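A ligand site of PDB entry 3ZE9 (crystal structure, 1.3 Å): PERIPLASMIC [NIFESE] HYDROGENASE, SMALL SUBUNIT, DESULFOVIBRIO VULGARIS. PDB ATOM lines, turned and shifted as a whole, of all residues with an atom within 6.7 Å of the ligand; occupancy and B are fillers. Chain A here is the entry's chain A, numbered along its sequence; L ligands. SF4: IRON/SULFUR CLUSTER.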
ATOM      1  N   ILE A 207      11.844  20.201  21.045  1.00  0.00           N
ATOM      2  CA  ILE A 207      11.194  19.822  19.804  1.00  0.00           C
ATOM      3  C   ILE A 207      10.992  18.302  19.728  1.00  0.00           C
ATOM      4  O   ILE A 207       9.883  17.799  19.541  1.00  0.00           O
ATOM      5  CB  ILE A 207      12.010  20.285  18.593  1.00  0.00           C
ATOM      6  CG1 ILE A 207      12.024  21.815  18.467  1.00  0.00           C
ATOM      7  CG2 ILE A 207      11.475  19.648  17.326  1.00  0.00           C
ATOM      8  CD1 ILE A 207      10.767  22.423  17.877  1.00  0.00           C
ATOM      9  N   HIS A 208      12.069  17.549  19.896  1.00  0.00           N
ATOM     10  CA  HIS A 208      12.045  16.110  19.650  1.00  0.00           C
ATOM     11  C   HIS A 208      11.119  15.347  20.596  1.00  0.00           C
ATOM     12  O   HIS A 208      10.364  14.463  20.169  1.00  0.00           O
ATOM     13  CB  HIS A 208      13.490  15.636  19.782  1.00  0.00           C
ATOM     14  CG  HIS A 208      13.697  14.159  19.750  1.00  0.00           C
ATOM     15  ND1 HIS A 208      13.670  13.409  18.596  1.00  0.00           N
ATOM     16  CD2 HIS A 208      13.977  13.296  20.759  1.00  0.00           C
ATOM     17  CE1 HIS A 208      13.938  12.149  18.883  1.00  0.00           C
ATOM     18  NE2 HIS A 208      14.119  12.053  20.190  1.00  0.00           N
ATOM     19  N   GLU A 209      11.169  15.671  21.895  1.00  0.00           N
ATOM     20  CA  GLU A 209      10.328  14.950  22.855  1.00  0.00           C
ATOM     21  C   GLU A 209       8.845  15.225  22.626  1.00  0.00           C
ATOM     22  O   GLU A 209       8.023  14.461  23.091  1.00  0.00           O
ATOM     23  CB  GLU A 209      10.734  15.264  24.301  1.00  0.00           C
ATOM     24  CG  GLU A 209      12.146  14.759  24.633  1.00  0.00           C
ATOM     25  CD  GLU A 209      12.324  13.244  24.488  1.00  0.00           C
ATOM     26  OE1 GLU A 209      11.332  12.490  24.570  1.00  0.00           O
ATOM     27  OE2 GLU A 209      13.478  12.776  24.282  1.00  0.00           O
ATOM     28  N   CYS A 211       7.709  15.705  19.353  1.00  0.00           N
ATOM     29  CA  CYS A 211       7.587  15.579  17.904  1.00  0.00           C
ATOM     30  C   CYS A 211       6.629  14.453  17.518  1.00  0.00           C
ATOM     31  O   CYS A 211       6.668  13.372  18.079  1.00  0.00           O
ATOM     32  CB  CYS A 211       8.963  15.312  17.275  1.00  0.00           C
ATOM     33  SG  CYS A 211       8.911  15.136  15.472  1.00  0.00           S
ATOM     34  N   PRO A 212       5.798  14.705  16.511  1.00  0.00           N
ATOM     35  CA  PRO A 212       4.879  13.639  16.108  1.00  0.00           C
ATOM     36  C   PRO A 212       5.536  12.424  15.450  1.00  0.00           C
ATOM     37  O   PRO A 212       4.886  11.408  15.251  1.00  0.00           O
ATOM     38  CB  PRO A 212       3.940  14.345  15.107  1.00  0.00           C
ATOM     39  CG  PRO A 212       4.707  15.531  14.614  1.00  0.00           C
ATOM     40  CD  PRO A 212       5.582  15.967  15.770  1.00  0.00           C
ATOM     41  N   TYR A 213       6.820  12.527  15.129  1.00  0.00           N
ATOM     42  CA  TYR A 213       7.539  11.401  14.546  1.00  0.00           C
ATOM     43  C   TYR A 213       8.404  10.655  15.549  1.00  0.00           C
ATOM     44  O   TYR A 213       9.166   9.769  15.180  1.00  0.00           O
ATOM     45  CB  TYR A 213       8.374  11.890  13.354  1.00  0.00           C
ATOM     46  CG  TYR A 213       7.481  12.490  12.313  1.00  0.00           C
ATOM     47  CD1 TYR A 213       6.623  11.684  11.591  1.00  0.00           C
ATOM     48  CD2 TYR A 213       7.456  13.851  12.097  1.00  0.00           C
ATOM     49  CE1 TYR A 213       5.768  12.223  10.648  1.00  0.00           C
ATOM     50  CE2 TYR A 213       6.604  14.397  11.150  1.00  0.00           C
ATOM     51  CZ  TYR A 213       5.756  13.579  10.436  1.00  0.00           C
ATOM     52  OH  TYR A 213       4.907  14.090   9.494  1.00  0.00           O
ATOM     53  N   LEU A 214       8.247  10.976  16.844  1.00  0.00           N
ATOM     54  CA  LEU A 214       9.074  10.375  17.873  1.00  0.00           C
ATOM     55  C   LEU A 214       8.908   8.858  17.896  1.00  0.00           C
ATOM     56  O   LEU A 214       9.870   8.125  18.177  1.00  0.00           O
ATOM     57  CB  LEU A 214       8.745  10.984  19.245  1.00  0.00           C
ATOM     58  CG  LEU A 214       9.540  10.444  20.441  1.00  0.00           C
ATOM     59  CD1 LEU A 214      11.010  10.775  20.301  1.00  0.00           C
ATOM     60  CD2 LEU A 214       9.007  11.063  21.727  1.00  0.00           C
ATOM     61  N   ASP A 215       7.710   8.354  17.613  1.00  0.00           N
ATOM     62  CA  ASP A 215       7.505   6.922  17.599  1.00  0.00           C
ATOM     63  C   ASP A 215       8.362   6.244  16.521  1.00  0.00           C
ATOM     64  O   ASP A 215       8.879   5.147  16.735  1.00  0.00           O
ATOM     65  CB  ASP A 215       6.022   6.538  17.464  1.00  0.00           C
ATOM     66  CG  ASP A 215       5.374   7.050  16.170  1.00  0.00           C
ATOM     67  OD1 ASP A 215       5.809   8.050  15.576  1.00  0.00           O
ATOM     68  OD2 ASP A 215       4.358   6.440  15.765  1.00  0.00           O
ATOM     69  N   LYS A 216       8.493   6.900  15.385  1.00  0.00           N
ATOM     70  CA  LYS A 216       9.286   6.374  14.301  1.00  0.00           C
ATOM     71  C   LYS A 216      10.773   6.416  14.670  1.00  0.00           C
ATOM     72  O   LYS A 216      11.515   5.483  14.377  1.00  0.00           O
ATOM     73  CB  LYS A 216       9.044   7.176  13.042  1.00  0.00           C
ATOM     74  CG  LYS A 216       7.615   7.100  12.532  1.00  0.00           C
ATOM     75  CD  LYS A 216       7.245   5.694  12.102  1.00  0.00           C
ATOM     76  CE  LYS A 216       5.811   5.641  11.669  1.00  0.00           C
ATOM     77  NZ  LYS A 216       5.407   4.271  11.296  1.00  0.00           N
ATOM     78  N   TYR A 217      11.206   7.494  15.297  1.00  0.00           N
ATOM     79  CA  TYR A 217      12.574   7.555  15.819  1.00  0.00           C
ATOM     80  C   TYR A 217      12.885   6.370  16.728  1.00  0.00           C
ATOM     81  O   TYR A 217      13.895   5.660  16.567  1.00  0.00           O
ATOM     82  CB  TYR A 217      12.758   8.862  16.596  1.00  0.00           C
ATOM     83  CG  TYR A 217      14.087   9.021  17.297  1.00  0.00           C
ATOM     84  CD1 TYR A 217      15.165   9.621  16.651  1.00  0.00           C
ATOM     85  CD2 TYR A 217      14.246   8.601  18.609  1.00  0.00           C
ATOM     86  CE1 TYR A 217      16.371   9.779  17.294  1.00  0.00           C
ATOM     87  CE2 TYR A 217      15.447   8.758  19.268  1.00  0.00           C
ATOM     88  CZ  TYR A 217      16.511   9.340  18.599  1.00  0.00           C
ATOM     89  OH  TYR A 217      17.716   9.505  19.254  1.00  0.00           O
ATOM     90  N   ASP A 218      11.981   6.114  17.683  1.00  0.00           N
ATOM     91  CA  ASP A 218      12.166   5.031  18.644  1.00  0.00           C
ATOM     92  C   ASP A 218      12.202   3.667  17.950  1.00  0.00           C
ATOM     93  O   ASP A 218      12.904   2.764  18.391  1.00  0.00           O
ATOM     94  CB  ASP A 218      11.057   5.057  19.703  1.00  0.00           C
ATOM     95  CG  ASP A 218      11.252   6.155  20.732  1.00  0.00           C
ATOM     96  OD1 ASP A 218      12.369   6.701  20.826  1.00  0.00           O
ATOM     97  OD2 ASP A 218      10.283   6.437  21.463  1.00  0.00           O
ATOM     98  N   MET A 222      13.460   5.526   9.571  1.00  0.00           N
ATOM     99  CA  MET A 222      14.019   6.782   9.136  1.00  0.00           C
ATOM    100  C   MET A 222      13.753   6.993   7.655  1.00  0.00           C
ATOM    101  O   MET A 222      14.030   6.123   6.827  1.00  0.00           O
ATOM    102  CB  MET A 222      15.537   6.754   9.301  1.00  0.00           C
ATOM    103  CG  MET A 222      15.990   6.562  10.710  1.00  0.00           C
ATOM    104  SD  MET A 222      15.556   8.009  11.673  1.00  0.00           S
ATOM    105  CE  MET A 222      15.950   7.418  13.337  1.00  0.00           C
ATOM    106  N   GLY A 231       8.524   8.580   7.915  1.00  0.00           N
ATOM    107  CA  GLY A 231       9.609   8.275   8.824  1.00  0.00           C
ATOM    108  C   GLY A 231      10.142   9.479   9.579  1.00  0.00           C
ATOM    109  O   GLY A 231       9.803  10.628   9.280  1.00  0.00           O
ATOM    110  N   CYS A 232      10.966   9.196  10.572  1.00  0.00           N
ATOM    111  CA  CYS A 232      11.697  10.220  11.286  1.00  0.00           C
ATOM    112  C   CYS A 232      12.769  10.820  10.374  1.00  0.00           C
ATOM    113  O   CYS A 232      13.289  10.141   9.472  1.00  0.00           O
ATOM    114  CB  CYS A 232      12.306   9.603  12.541  1.00  0.00           C
ATOM    115  SG  CYS A 232      13.588  10.559  13.376  1.00  0.00           S
ATOM    116  N   ARG A 233      13.079  12.092  10.608  1.00  0.00           N
ATOM    117  CA  ARG A 233      13.978  12.880   9.770  1.00  0.00           C
ATOM    118  C   ARG A 233      15.421  12.893  10.293  1.00  0.00           C
ATOM    119  O   ARG A 233      16.273  13.620   9.787  1.00  0.00           O
ATOM    120  CB  ARG A 233      13.474  14.315   9.658  1.00  0.00           C
ATOM    121  CG  ARG A 233      12.252  14.547   8.768  1.00  0.00           C
ATOM    122  CD  ARG A 233      10.948  13.935   9.273  1.00  0.00           C
ATOM    123  NE  ARG A 233       9.815  14.651   8.692  1.00  0.00           N
ATOM    124  CZ  ARG A 233       8.621  14.141   8.445  1.00  0.00           C
ATOM    125  NH1 ARG A 233       8.343  12.873   8.700  1.00  0.00           N
ATOM    126  NH2 ARG A 233       7.683  14.932   7.916  1.00  0.00           N
ATOM    127  N   TYR A 234      15.720  12.085  11.304  1.00  0.00           N
ATOM    128  CA  TYR A 234      17.020  12.141  11.957  1.00  0.00           C
ATOM    129  C   TYR A 234      18.175  11.860  10.990  1.00  0.00           C
ATOM    130  O   TYR A 234      19.187  12.562  11.007  1.00  0.00           O
ATOM    131  CB  TYR A 234      17.069  11.171  13.131  1.00  0.00           C
ATOM    132  CG  TYR A 234      18.386  11.153  13.864  1.00  0.00           C
ATOM    133  CD1 TYR A 234      18.650  12.091  14.846  1.00  0.00           C
ATOM    134  CD2 TYR A 234      19.363  10.230  13.565  1.00  0.00           C
ATOM    135  CE1 TYR A 234      19.851  12.097  15.523  1.00  0.00           C
ATOM    136  CE2 TYR A 234      20.582  10.232  14.230  1.00  0.00           C
ATOM    137  CZ  TYR A 234      20.809  11.176  15.213  1.00  0.00           C
ATOM    138  OH  TYR A 234      22.004  11.180  15.883  1.00  0.00           O
ATOM    139  N   ASP A 235      18.054  10.834  10.147  1.00  0.00           N
ATOM    140  CA  ASP A 235      19.146  10.524   9.209  1.00  0.00           C
ATOM    141  C   ASP A 235      19.327  11.608   8.140  1.00  0.00           C
ATOM    142  O   ASP A 235      20.411  11.732   7.560  1.00  0.00           O
ATOM    143  CB  ASP A 235      18.905   9.177   8.511  1.00  0.00           C
ATOM    144  CG  ASP A 235      19.147   7.976   9.399  1.00  0.00           C
ATOM    145  OD1 ASP A 235      19.632   8.112  10.536  1.00  0.00           O
ATOM    146  OD2 ASP A 235      18.841   6.851   8.926  1.00  0.00           O
ATOM    147  N   CYS A 238      17.915  16.043  10.932  1.00  0.00           N
ATOM    148  CA  CYS A 238      17.093  16.770  11.908  1.00  0.00           C
ATOM    149  C   CYS A 238      17.824  16.974  13.237  1.00  0.00           C
ATOM    150  O   CYS A 238      18.319  16.019  13.852  1.00  0.00           O
ATOM    151  CB  CYS A 238      15.790  16.015  12.144  1.00  0.00           C
ATOM    152  SG  CYS A 238      14.648  16.947  13.188  1.00  0.00           S
ATOM    153  N   LYS A 239      17.827  18.233  13.715  1.00  0.00           N
ATOM    154  CA  LYS A 239      18.462  18.587  14.986  1.00  0.00           C
ATOM    155  C   LYS A 239      17.434  18.799  16.112  1.00  0.00           C
ATOM    156  O   LYS A 239      17.766  19.349  17.169  1.00  0.00           O
ATOM    157  CB  LYS A 239      19.311  19.842  14.813  1.00  0.00           C
ATOM    158  CG  LYS A 239      20.400  19.688  13.731  1.00  0.00           C
ATOM    159  CD  LYS A 239      21.246  18.441  13.910  1.00  0.00           C
ATOM    160  CE  LYS A 239      22.478  18.403  12.975  1.00  0.00           C
ATOM    161  NZ  LYS A 239      22.101  18.626  11.553  1.00  0.00           N
ATOM    162  N   GLY A 240      16.200  18.340  15.898  1.00  0.00           N
ATOM    163  CA  GLY A 240      15.187  18.409  16.938  1.00  0.00           C
ATOM    164  C   GLY A 240      15.639  17.948  18.311  1.00  0.00           C
ATOM    165  O   GLY A 240      15.273  18.555  19.326  1.00  0.00           O
ATOM    166  N   PRO A 241      16.406  16.862  18.403  1.00  0.00           N
ATOM    167  CA  PRO A 241      16.804  16.417  19.738  1.00  0.00           C
ATOM    168  C   PRO A 241      17.541  17.453  20.586  1.00  0.00           C
ATOM    169  O   PRO A 241      17.439  17.457  21.811  1.00  0.00           O
ATOM    170  CB  PRO A 241      17.716  15.211  19.457  1.00  0.00           C
ATOM    171  CG  PRO A 241      17.195  14.686  18.157  1.00  0.00           C
ATOM    172  CD  PRO A 241      16.823  15.911  17.353  1.00  0.00           C
ATOM    173  N   TRP A 258       5.785  23.605   9.258  1.00  0.00           N
ATOM    174  CA  TRP A 258       6.944  23.843  10.089  1.00  0.00           C
ATOM    175  C   TRP A 258       8.109  23.001   9.588  1.00  0.00           C
ATOM    176  O   TRP A 258       7.932  22.158   8.712  1.00  0.00           O
ATOM    177  CB  TRP A 258       6.670  23.583  11.580  1.00  0.00           C
ATOM    178  CG  TRP A 258       6.419  22.164  11.985  1.00  0.00           C
ATOM    179  CD1 TRP A 258       5.405  21.351  11.555  1.00  0.00           C
ATOM    180  CD2 TRP A 258       7.141  21.415  12.972  1.00  0.00           C
ATOM    181  NE1 TRP A 258       5.469  20.132  12.201  1.00  0.00           N
ATOM    182  CE2 TRP A 258       6.531  20.154  13.074  1.00  0.00           C
ATOM    183  CE3 TRP A 258       8.249  21.685  13.773  1.00  0.00           C
ATOM    184  CZ2 TRP A 258       7.004  19.165  13.958  1.00  0.00           C
ATOM    185  CZ3 TRP A 258       8.695  20.711  14.661  1.00  0.00           C
ATOM    186  CH2 TRP A 258       8.080  19.463  14.739  1.00  0.00           C
ATOM    187  N   VAL A 260      10.186  20.617  10.586  1.00  0.00           N
ATOM    188  CA  VAL A 260      10.256  19.161  10.631  1.00  0.00           C
ATOM    189  C   VAL A 260       9.272  18.510   9.681  1.00  0.00           C
ATOM    190  O   VAL A 260       9.604  17.497   9.019  1.00  0.00           O
ATOM    191  CB  VAL A 260      10.057  18.655  12.060  1.00  0.00           C
ATOM    192  CG1 VAL A 260       9.954  17.153  12.096  1.00  0.00           C
ATOM    193  CG2 VAL A 260      11.200  19.160  12.928  1.00  0.00           C
ATOM    194  N   ALA A 263      10.910  19.532   5.999  1.00  0.00           N
ATOM    195  CA  ALA A 263      12.282  19.126   5.712  1.00  0.00           C
ATOM    196  C   ALA A 263      12.915  18.632   7.026  1.00  0.00           C
ATOM    197  O   ALA A 263      12.550  17.544   7.480  1.00  0.00           O
ATOM    198  CB  ALA A 263      13.064  20.275   5.059  1.00  0.00           C
ATOM    199  N   VAL A 264      13.828  19.390   7.624  1.00  0.00           N
ATOM    200  CA  VAL A 264      14.445  19.067   8.917  1.00  0.00           C
ATOM    201  C   VAL A 264      14.525  20.308   9.776  1.00  0.00           C
ATOM    202  O   VAL A 264      14.503  21.430   9.258  1.00  0.00           O
ATOM    203  CB  VAL A 264      15.891  18.513   8.716  1.00  0.00           C
ATOM    204  CG1 VAL A 264      15.869  17.234   7.884  1.00  0.00           C
ATOM    205  CG2 VAL A 264      16.779  19.534   8.058  1.00  0.00           C
ATOM    206  N   CYS A 265      14.596  20.122  11.096  1.00  0.00           N
ATOM    207  CA  CYS A 265      15.014  21.216  11.977  1.00  0.00           C
ATOM    208  C   CYS A 265      16.523  21.420  11.909  1.00  0.00           C
ATOM    209  O   CYS A 265      17.291  20.442  11.928  1.00  0.00           O
ATOM    210  CB  CYS A 265      14.592  20.885  13.418  1.00  0.00           C
ATOM    211  SG  CYS A 265      15.079  22.084  14.712  1.00  0.00           S
HETATM  212 FE1  SF4 L   1      13.507  15.225  14.263  1.00  0.00          FE
HETATM  213 FE2  SF4 L   1      13.224  13.879  16.637  1.00  0.00          FE
HETATM  214 FE3  SF4 L   1      12.837  12.513  14.331  1.00  0.00          FE
HETATM  215 FE4  SF4 L   1      11.060  14.427  15.149  1.00  0.00          FE
HETATM  216  S1  SF4 L   1      11.495  12.417  16.178  1.00  0.00           S
HETATM  217  S2  SF4 L   1      12.471  15.989  16.147  1.00  0.00           S
HETATM  218  S3  SF4 L   1      11.854  14.117  13.030  1.00  0.00           S
HETATM  219  S4  SF4 L   1      14.822  13.496  15.034  1.00  0.00           S
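SG of Cys 232 is bound to FE3 of the ligand, 2.3 Å away.
S1 of the ligand sits close to N of Leu 214 (3.6 Å).
A sulfur (S3) of the ligand sits close to the backbone NH (N) of Arg 233, 3.4 Å away.
SG of Cys 211 is bound to FE4 of the ligand (2.3 Å).
ND1 of His 208 binds FE2 of the ligand.
An iron atom (FE1) of the ligand is bound by the side-chain sulfur of Cys 238, at 2.3 Å.
The backbone carbonyl oxygen of Tyr 213 sits close to a sulfur (S1) of the ligand (3.7 Å).
Ile 207 touches the ligand (CG2 to S2, 3.97 Å).
CB of Tyr 217 touches S1 of the ligand, 3.8 Å away.
Tyr 234 touches the ligand.
CA of Gly 240 touches S2 of the ligand, at 3.7 Å.
Pro 241 touches the ligand.
Val 260 touches the ligand (CG1 to S3, 3.7 Å).
Hydrophobic or aromatic side chains that line the ligand: Ile 207, His 208, Tyr 217, Tyr 234, Pro 241 and Val 260.
Along chain A the residues within 4 Å of the ligand span positions 207 to 260.
The nearest printed residue that does not touch the ligand is Lys 239 (5.3 Å).
The side-chain sulfur (SG) of Cys 238 sits close to the backbone NH (N) of Gly 240, at 3.4 Å.
The backbone NH (N) of His 208 is in hydrogen-bond range of the backbone carbonyl oxygen (O) of Gly 240, at 3.4 Å.
The backbone NH of Tyr 213 sits close to the side-chain sulfur of Cys 211, 3.4 Å away.
The backbone NH (N) of Tyr 234 sits close to the side-chain sulfur (SG) of Cys 232, 3.3 Å away.
NH1 of Arg 233 sits at hydrogen-bond distance from O of Gly 231, at 2.7 Å.
O of Arg 233 is in hydrogen-bond range of N of Cys 238, at 3.1 Å.
The side-chain hydroxyl of Tyr 213 lies within hydrogen-bond range of the guanidinium group of Arg 233.
The side-chain sulfur (SG) of Cys 232 lies close to the side-chain sulfur (SD) of Met 222.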
